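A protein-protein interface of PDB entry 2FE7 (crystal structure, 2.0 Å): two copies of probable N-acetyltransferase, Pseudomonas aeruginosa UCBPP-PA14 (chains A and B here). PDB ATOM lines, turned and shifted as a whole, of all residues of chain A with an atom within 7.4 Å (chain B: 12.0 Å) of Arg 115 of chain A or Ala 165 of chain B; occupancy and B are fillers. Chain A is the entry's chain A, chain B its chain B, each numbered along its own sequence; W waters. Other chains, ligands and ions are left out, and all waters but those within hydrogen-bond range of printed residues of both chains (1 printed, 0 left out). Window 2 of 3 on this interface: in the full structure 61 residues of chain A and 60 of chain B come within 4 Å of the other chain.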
ATOM      1  N   ILE A  89       0.333  18.254  21.624  1.00  0.00           N
ATOM      2  CA  ILE A  89       1.101  19.429  21.205  1.00  0.00           C
ATOM      3  C   ILE A  89       2.192  18.974  20.255  1.00  0.00           C
ATOM      4  O   ILE A  89       2.857  17.959  20.507  1.00  0.00           O
ATOM      5  CB  ILE A  89       1.732  20.165  22.397  1.00  0.00           C
ATOM      6  CG1 ILE A  89       0.621  20.706  23.317  1.00  0.00           C
ATOM      7  CG2 ILE A  89       2.661  21.288  21.909  1.00  0.00           C
ATOM      8  CD1 ILE A  89       1.116  21.458  24.543  1.00  0.00           C
ATOM      9  N   ARG A 108      14.443  23.165  30.095  1.00  0.00           N
ATOM     10  CA  ARG A 108      13.478  24.033  30.750  1.00  0.00           C
ATOM     11  C   ARG A 108      12.301  24.386  29.832  1.00  0.00           C
ATOM     12  O   ARG A 108      11.143  24.347  30.254  1.00  0.00           O
ATOM     13  CB  ARG A 108      14.183  25.302  31.224  1.00  0.00           C
ATOM     14  CG  ARG A 108      13.379  26.125  32.175  1.00  0.00           C
ATOM     15  CD  ARG A 108      13.510  25.606  33.597  1.00  0.00           C
ATOM     16  NE  ARG A 108      12.367  26.024  34.403  1.00  0.00           N
ATOM     17  CZ  ARG A 108      12.136  27.275  34.801  1.00  0.00           C
ATOM     18  NH1 ARG A 108      12.971  28.257  34.475  1.00  0.00           N
ATOM     19  NH2 ARG A 108      11.060  27.542  35.532  1.00  0.00           N
ATOM     20  N   LEU A 109      12.602  24.727  28.580  1.00  0.00           N
ATOM     21  CA  LEU A 109      11.565  24.997  27.581  1.00  0.00           C
ATOM     22  C   LEU A 109      10.676  23.769  27.357  1.00  0.00           C
ATOM     23  O   LEU A 109       9.446  23.889  27.313  1.00  0.00           O
ATOM     24  CB  LEU A 109      12.184  25.465  26.259  1.00  0.00           C
ATOM     25  CG  LEU A 109      12.647  26.920  26.126  1.00  0.00           C
ATOM     26  CD1 LEU A 109      13.611  27.091  24.947  1.00  0.00           C
ATOM     27  CD2 LEU A 109      11.466  27.885  25.998  1.00  0.00           C
ATOM     28  N   LEU A 110      11.296  22.595  27.244  1.00  0.00           N
ATOM     29  CA  LEU A 110      10.550  21.333  27.099  1.00  0.00           C
ATOM     30  C   LEU A 110       9.645  21.021  28.284  1.00  0.00           C
ATOM     31  O   LEU A 110       8.516  20.540  28.104  1.00  0.00           O
ATOM     32  CB  LEU A 110      11.492  20.155  26.842  1.00  0.00           C
ATOM     33  CG  LEU A 110      11.797  19.817  25.384  1.00  0.00           C
ATOM     34  CD1 LEU A 110      12.964  18.870  25.312  1.00  0.00           C
ATOM     35  CD2 LEU A 110      10.587  19.211  24.677  1.00  0.00           C
ATOM     36  N   ARG A 111      10.149  21.288  29.486  1.00  0.00           N
ATOM     37  CA  ARG A 111       9.397  21.074  30.717  1.00  0.00           C
ATOM     38  C   ARG A 111       8.108  21.890  30.699  1.00  0.00           C
ATOM     39  O   ARG A 111       7.033  21.372  31.009  1.00  0.00           O
ATOM     40  CB  ARG A 111      10.258  21.450  31.928  1.00  0.00           C
ATOM     41  CG  ARG A 111       9.594  21.314  33.296  1.00  0.00           C
ATOM     42  CD  ARG A 111      10.653  21.353  34.408  1.00  0.00           C
ATOM     43  NE  ARG A 111      11.615  20.253  34.241  1.00  0.00           N
ATOM     44  CZ  ARG A 111      12.902  20.382  33.889  1.00  0.00           C
ATOM     45  NH1 ARG A 111      13.451  21.583  33.684  1.00  0.00           N
ATOM     46  NH2 ARG A 111      13.656  19.288  33.757  1.00  0.00           N
ATOM     47  N   GLU A 112       8.230  23.162  30.315  1.00  0.00           N
ATOM     48  CA  GLU A 112       7.082  24.058  30.229  1.00  0.00           C
ATOM     49  C   GLU A 112       6.055  23.564  29.225  1.00  0.00           C
ATOM     50  O   GLU A 112       4.850  23.622  29.487  1.00  0.00           O
ATOM     51  CB  GLU A 112       7.529  25.491  29.911  1.00  0.00           C
ATOM     52  CG  GLU A 112       8.260  26.155  31.074  1.00  0.00           C
ATOM     53  CD  GLU A 112       7.474  26.103  32.378  1.00  0.00           C
ATOM     54  OE1 GLU A 112       6.339  26.632  32.409  1.00  0.00           O
ATOM     55  OE2 GLU A 112       7.987  25.532  33.370  1.00  0.00           O
ATOM     56  N   LEU A 113       6.538  23.050  28.097  1.00  0.00           N
ATOM     57  CA  LEU A 113       5.659  22.477  27.070  1.00  0.00           C
ATOM     58  C   LEU A 113       4.942  21.238  27.590  1.00  0.00           C
ATOM     59  O   LEU A 113       3.740  21.070  27.359  1.00  0.00           O
ATOM     60  CB  LEU A 113       6.432  22.173  25.779  1.00  0.00           C
ATOM     61  CG  LEU A 113       6.905  23.432  25.040  1.00  0.00           C
ATOM     62  CD1 LEU A 113       8.061  23.144  24.117  1.00  0.00           C
ATOM     63  CD2 LEU A 113       5.751  24.085  24.282  1.00  0.00           C
ATOM     64  N   ALA A 114       5.680  20.386  28.305  1.00  0.00           N
ATOM     65  CA  ALA A 114       5.102  19.192  28.930  1.00  0.00           C
ATOM     66  C   ALA A 114       4.040  19.569  29.969  1.00  0.00           C
ATOM     67  O   ALA A 114       2.951  18.986  30.005  1.00  0.00           O
ATOM     68  CB  ALA A 114       6.199  18.334  29.552  1.00  0.00           C
ATOM     69  N   ARG A 115       4.349  20.560  30.805  1.00  0.00           N
ATOM     70  CA  ARG A 115       3.377  21.071  31.777  1.00  0.00           C
ATOM     71  C   ARG A 115       2.121  21.589  31.075  1.00  0.00           C
ATOM     72  O   ARG A 115       1.004  21.342  31.524  1.00  0.00           O
ATOM     73  CB  ARG A 115       3.992  22.176  32.638  1.00  0.00           C
ATOM     74  CG  ARG A 115       5.088  21.706  33.581  1.00  0.00           C
ATOM     75  CD  ARG A 115       5.560  22.829  34.502  1.00  0.00           C
ATOM     76  NE  ARG A 115       4.631  23.050  35.610  1.00  0.00           N
ATOM     77  CZ  ARG A 115       3.734  24.035  35.670  1.00  0.00           C
ATOM     78  NH1 ARG A 115       3.636  24.926  34.685  1.00  0.00           N
ATOM     79  NH2 ARG A 115       2.936  24.134  36.727  1.00  0.00           N
ATOM     80  N   GLU A 116       2.312  22.299  29.963  1.00  0.00           N
ATOM     81  CA  GLU A 116       1.189  22.777  29.172  1.00  0.00           C
ATOM     82  C   GLU A 116       0.385  21.581  28.642  1.00  0.00           C
ATOM     83  O   GLU A 116      -0.841  21.584  28.703  1.00  0.00           O
ATOM     84  CB  GLU A 116       1.651  23.692  28.023  1.00  0.00           C
ATOM     85  CG  GLU A 116       0.480  24.314  27.252  1.00  0.00           C
ATOM     86  CD  GLU A 116       0.906  25.248  26.123  1.00  0.00           C
ATOM     87  OE1 GLU A 116       1.989  25.884  26.221  1.00  0.00           O
ATOM     88  OE2 GLU A 116       0.138  25.359  25.133  1.00  0.00           O
ATOM     89  N   ALA A 117       1.089  20.554  28.156  1.00  0.00           N
ATOM     90  CA  ALA A 117       0.455  19.333  27.640  1.00  0.00           C
ATOM     91  C   ALA A 117      -0.389  18.652  28.722  1.00  0.00           C
ATOM     92  O   ALA A 117      -1.548  18.321  28.495  1.00  0.00           O
ATOM     93  CB  ALA A 117       1.516  18.370  27.081  1.00  0.00           C
ATOM     94  N   VAL A 118       0.186  18.484  29.907  1.00  0.00           N
ATOM     95  CA  VAL A 118      -0.520  17.874  31.042  1.00  0.00           C
ATOM     96  C   VAL A 118      -1.746  18.692  31.497  1.00  0.00           C
ATOM     97  O   VAL A 118      -2.834  18.139  31.678  1.00  0.00           O
ATOM     98  CB  VAL A 118       0.471  17.547  32.207  1.00  0.00           C
ATOM     99  CG1 VAL A 118      -0.259  17.187  33.479  1.00  0.00           C
ATOM    100  CG2 VAL A 118       1.394  16.401  31.793  1.00  0.00           C
ATOM    101  N   ALA A 119      -1.586  20.006  31.637  1.00  0.00           N
ATOM    102  CA  ALA A 119      -2.689  20.872  32.080  1.00  0.00           C
ATOM    103  C   ALA A 119      -3.826  20.932  31.057  1.00  0.00           C
ATOM    104  O   ALA A 119      -4.997  21.033  31.430  1.00  0.00           O
ATOM    105  CB  ALA A 119      -2.180  22.273  32.395  1.00  0.00           C
ATOM    106  N   ASN A 120      -3.478  20.857  29.774  1.00  0.00           N
ATOM    107  CA  ASN A 120      -4.470  20.904  28.705  1.00  0.00           C
ATOM    108  C   ASN A 120      -4.961  19.533  28.240  1.00  0.00           C
ATOM    109  O   ASN A 120      -5.480  19.406  27.133  1.00  0.00           O
ATOM    110  CB  ASN A 120      -3.960  21.718  27.517  1.00  0.00           C
ATOM    111  CG  ASN A 120      -4.024  23.215  27.753  1.00  0.00           C
ATOM    112  OD1 ASN A 120      -3.034  23.916  27.573  1.00  0.00           O
ATOM    113  ND2 ASN A 120      -5.181  23.709  28.154  1.00  0.00           N
ATOM    114  N   ASP A 121      -4.808  18.518  29.087  1.00  0.00           N
ATOM    115  CA  ASP A 121      -5.331  17.176  28.799  1.00  0.00           C
ATOM    116  C   ASP A 121      -4.765  16.559  27.509  1.00  0.00           C
ATOM    117  O   ASP A 121      -5.487  15.884  26.773  1.00  0.00           O
ATOM    118  CB  ASP A 121      -6.869  17.215  28.739  1.00  0.00           C
ATOM    119  CG  ASP A 121      -7.507  15.838  28.884  1.00  0.00           C
ATOM    120  OD1 ASP A 121      -6.852  14.912  29.404  1.00  0.00           O
ATOM    121  OD2 ASP A 121      -8.672  15.686  28.463  1.00  0.00           O
ATOM    122  N   LEU A 125       3.349  14.850  23.413  1.00  0.00           N
ATOM    123  CA  LEU A 125       4.177  15.982  23.003  1.00  0.00           C
ATOM    124  C   LEU A 125       5.113  15.427  21.934  1.00  0.00           C
ATOM    125  O   LEU A 125       5.766  14.412  22.163  1.00  0.00           O
ATOM    126  CB  LEU A 125       4.971  16.518  24.190  1.00  0.00           C
ATOM    127  CG  LEU A 125       5.948  17.680  23.968  1.00  0.00           C
ATOM    128  CD1 LEU A 125       5.294  18.879  23.264  1.00  0.00           C
ATOM    129  CD2 LEU A 125       6.595  18.104  25.289  1.00  0.00           C
ATOM    130  N   ARG B 155       8.438  11.387  20.100  1.00  0.00           N
ATOM    131  CA  ARG B 155       7.245  11.482  20.927  1.00  0.00           C
ATOM    132  C   ARG B 155       7.548  11.249  22.408  1.00  0.00           C
ATOM    133  O   ARG B 155       8.284  10.323  22.767  1.00  0.00           O
ATOM    134  CB  ARG B 155       6.207  10.453  20.452  1.00  0.00           C
ATOM    135  CG  ARG B 155       4.940  10.391  21.283  1.00  0.00           C
ATOM    136  CD  ARG B 155       4.062   9.217  20.884  1.00  0.00           C
ATOM    137  NE  ARG B 155       3.528   9.407  19.539  1.00  0.00           N
ATOM    138  CZ  ARG B 155       2.741   8.537  18.909  1.00  0.00           C
ATOM    139  NH1 ARG B 155       2.312   8.808  17.689  1.00  0.00           N
ATOM    140  NH2 ARG B 155       2.394   7.400  19.494  1.00  0.00           N
ATOM    141  N   LEU B 156       6.971  12.108  23.249  1.00  0.00           N
ATOM    142  CA  LEU B 156       6.873  11.861  24.682  1.00  0.00           C
ATOM    143  C   LEU B 156       5.412  11.619  25.002  1.00  0.00           C
ATOM    144  O   LEU B 156       4.565  12.446  24.688  1.00  0.00           O
ATOM    145  CB  LEU B 156       7.321  13.078  25.485  1.00  0.00           C
ATOM    146  CG  LEU B 156       8.776  13.399  25.792  1.00  0.00           C
ATOM    147  CD1 LEU B 156       8.793  14.714  26.568  1.00  0.00           C
ATOM    148  CD2 LEU B 156       9.452  12.287  26.591  1.00  0.00           C
ATOM    149  N   ASP B 157       5.114  10.491  25.635  1.00  0.00           N
ATOM    150  CA  ASP B 157       3.756  10.224  26.100  1.00  0.00           C
ATOM    151  C   ASP B 157       3.808   9.399  27.384  1.00  0.00           C
ATOM    152  O   ASP B 157       4.899   9.088  27.879  1.00  0.00           O
ATOM    153  CB  ASP B 157       2.900   9.577  24.991  1.00  0.00           C
ATOM    154  CG  ASP B 157       3.383   8.182  24.590  1.00  0.00           C
ATOM    155  OD1 ASP B 157       2.799   7.591  23.651  1.00  0.00           O
ATOM    156  OD2 ASP B 157       4.332   7.668  25.213  1.00  0.00           O
ATOM    157  N   GLY B 158       2.641   9.070  27.933  1.00  0.00           N
ATOM    158  CA  GLY B 158       2.562   8.244  29.141  1.00  0.00           C
ATOM    159  C   GLY B 158       3.431   8.758  30.270  1.00  0.00           C
ATOM    160  O   GLY B 158       3.422   9.952  30.568  1.00  0.00           O
ATOM    161  N   GLU B 159       4.195   7.861  30.893  1.00  0.00           N
ATOM    162  CA  GLU B 159       4.980   8.214  32.082  1.00  0.00           C
ATOM    163  C   GLU B 159       6.116   9.186  31.746  1.00  0.00           C
ATOM    164  O   GLU B 159       6.392  10.105  32.515  1.00  0.00           O
ATOM    165  CB  GLU B 159       5.488   6.955  32.818  1.00  0.00           C
ATOM    166  CG  GLU B 159       6.349   7.234  34.069  1.00  0.00           C
ATOM    167  CD  GLU B 159       6.506   6.030  35.011  1.00  0.00           C
ATOM    168  OE1 GLU B 159       7.666   5.594  35.232  1.00  0.00           O
ATOM    169  OE2 GLU B 159       5.484   5.534  35.558  1.00  0.00           O
ATOM    170  N   ALA B 160       6.761   8.993  30.593  1.00  0.00           N
ATOM    171  CA  ALA B 160       7.862   9.863  30.178  1.00  0.00           C
ATOM    172  C   ALA B 160       7.404  11.328  30.051  1.00  0.00           C
ATOM    173  O   ALA B 160       8.136  12.241  30.443  1.00  0.00           O
ATOM    174  CB  ALA B 160       8.497   9.363  28.871  1.00  0.00           C
ATOM    175  N   LEU B 161       6.193  11.537  29.534  1.00  0.00           N
ATOM    176  CA  LEU B 161       5.609  12.881  29.449  1.00  0.00           C
ATOM    177  C   LEU B 161       5.325  13.475  30.836  1.00  0.00           C
ATOM    178  O   LEU B 161       5.664  14.635  31.096  1.00  0.00           O
ATOM    179  CB  LEU B 161       4.327  12.877  28.607  1.00  0.00           C
ATOM    180  CG  LEU B 161       3.596  14.211  28.386  1.00  0.00           C
ATOM    181  CD1 LEU B 161       4.501  15.229  27.678  1.00  0.00           C
ATOM    182  CD2 LEU B 161       2.292  14.011  27.613  1.00  0.00           C
ATOM    183  N   ARG B 162       4.688  12.686  31.703  1.00  0.00           N
ATOM    184  CA  ARG B 162       4.397  13.099  33.081  1.00  0.00           C
ATOM    185  C   ARG B 162       5.666  13.514  33.820  1.00  0.00           C
ATOM    186  O   ARG B 162       5.700  14.573  34.445  1.00  0.00           O
ATOM    187  CB  ARG B 162       3.681  11.984  33.861  1.00  0.00           C
ATOM    188  CG  ARG B 162       2.223  11.738  33.450  1.00  0.00           C
ATOM    189  CD  ARG B 162       1.666  10.435  34.065  1.00  0.00           C
ATOM    190  NE  ARG B 162       0.953   9.635  33.064  1.00  0.00           N
ATOM    191  CZ  ARG B 162       1.032   8.308  32.954  1.00  0.00           C
ATOM    192  NH1 ARG B 162       1.790   7.601  33.790  1.00  0.00           N
ATOM    193  NH2 ARG B 162       0.353   7.684  31.996  1.00  0.00           N
ATOM    194  N   LYS B 163       6.701  12.679  33.743  1.00  0.00           N
ATOM    195  CA  LYS B 163       8.005  12.970  34.362  1.00  0.00           C
ATOM    196  C   LYS B 163       8.663  14.255  33.825  1.00  0.00           C
ATOM    197  O   LYS B 163       9.247  15.014  34.592  1.00  0.00           O
ATOM    198  CB  LYS B 163       8.962  11.774  34.212  1.00  0.00           C
ATOM    199  CG  LYS B 163       8.554  10.509  34.992  1.00  0.00           C
ATOM    200  CD  LYS B 163       8.945  10.588  36.473  1.00  0.00           C
ATOM    201  CE  LYS B 163       8.813   9.235  37.175  1.00  0.00           C
ATOM    202  NZ  LYS B 163       9.089   9.338  38.651  1.00  0.00           N
ATOM    203  N   MET B 164       8.566  14.494  32.515  1.00  0.00           N
ATOM    204  CA  MET B 164       9.066  15.741  31.915  1.00  0.00           C
ATOM    205  C   MET B 164       8.359  16.974  32.504  1.00  0.00           C
ATOM    206  O   MET B 164       8.974  18.020  32.682  1.00  0.00           O
ATOM    207  CB  MET B 164       8.930  15.715  30.386  1.00  0.00           C
ATOM    208  CG  MET B 164       9.736  16.800  29.651  1.00  0.00           C
ATOM    209  SD  MET B 164      11.514  16.500  29.647  1.00  0.00           S
ATOM    210  CE  MET B 164      12.105  18.038  30.358  1.00  0.00           C
ATOM    211  N   ALA B 165       7.074  16.839  32.818  1.00  0.00           N
ATOM    212  CA  ALA B 165       6.308  17.929  33.429  1.00  0.00           C
ATOM    213  C   ALA B 165       6.555  18.086  34.941  1.00  0.00           C
ATOM    214  O   ALA B 165       6.469  19.193  35.475  1.00  0.00           O
ATOM    215  CB  ALA B 165       4.826  17.755  33.145  1.00  0.00           C
ATOM    216  N   GLU B 166       6.857  16.978  35.618  1.00  0.00           N
ATOM    217  CA  GLU B 166       6.997  16.954  37.083  1.00  0.00           C
ATOM    218  C   GLU B 166       8.429  17.197  37.563  1.00  0.00           C
ATOM    219  O   GLU B 166       9.353  17.382  36.760  1.00  0.00           O
ATOM    220  CB  GLU B 166       6.473  15.633  37.654  1.00  0.00           C
ATOM    221  CG  GLU B 166       4.970  15.403  37.454  1.00  0.00           C
ATOM    222  CD  GLU B 166       4.467  14.082  38.040  1.00  0.00           C
ATOM    223  OE1 GLU B 166       5.287  13.309  38.600  1.00  0.00           O
ATOM    224  OE2 GLU B 166       3.242  13.820  37.936  1.00  0.00           O
HETATM  225  O   HOH W   1       7.775  22.075  36.667  1.00  0.00           O
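N of Leu 156 of chain B lies within hydrogen-bond range of O of Leu 125 of chain A (2.8 Å).
NH1 of Arg 115 of chain A lies within salt-bridge range of OE1 of Glu 112 of chain A, at 3.9 Å.
Among the printed residues, pairs that only touch across the chains: Arg 111 of chain A with Met 164 of chain B (3.4 Å), Arg 115 of chain A with Ala 165 of chain B (3.4 Å), Leu 125 of chain A with Arg 155 of chain B (3.5 Å), Ala 114 of chain A with Ala 165 of chain B (3.7 Å), Leu 125 of chain A with Leu 161 of chain B (3.7 Å), Ala 114 of chain A with Met 164 of chain B (3.9 Å) and Val 118 of chain A with Ala 165 of chain B (3.9 Å).
Of chain B, only Ala 165 comes within 4 Å of Arg 115 of chain A.
Ala 165 of chain B touches three residues of chain A.
Arg 111 of chain A touches one residue of chain B.
No residue of chain B comes within 4 Å of Glu 116 of chain A.
Val 118 of chain A touches one residue of chain B.
No residue of chain B comes within 4 Å of Ala 119 of chain A.
Of the printed residues of chain B, Ala 114 of chain A touches Met 164 (3.9 Å) and Ala 165 (3.7 Å).
Of the printed residues of chain A, Met 164 of chain B touches Arg 111 (3.4 Å) and Ala 114 (3.9 Å).
Of the printed residues of chain A, Arg 155 of chain B touches Leu 125.
Of the printed residues of chain A, Leu 156 of chain B touches Leu 125 (2.8 Å).
Of the printed residues of chain B, Leu 125 of chain A touches Arg 155 (3.5 Å), Leu 156 (2.8 Å) and Leu 161 (3.7 Å).
The nearest residue of chain A that does not touch Ala 165 of chain B is Arg 111 of chain A (4.3 Å).
The nearest printed residue of chain B that does not touch Leu 125 of chain A is Asp 157 of chain B (5.2 Å).
Printed residues of chain A that touch a printed residue of chain B: Arg 111, Ala 114, Arg 115, Val 118 and Leu 125.
Along chain A the printed residues that touch a printed residue of chain B span positions 111 to 125.
Printed residues of chain B that touch a printed residue of chain A: Arg 155, Leu 156, Leu 161, Met 164 and Ala 165.
Hydrophobic or aromatic side chains of chain B that line the printed part of chain A: Leu 156, Leu 161, Met 164 and Ala 165.
Among the printed residues, 8 pairs touch across the chains.
No position is printed for both chains.
Of the 8 pairs that touch across the chains among the printed residues, none has its exchanged pair printed and touching as well.
Water W1 bridges O of Ala 165 of chain B (3.4 Å) and NE of Arg 115 of chain A (3.5 Å).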
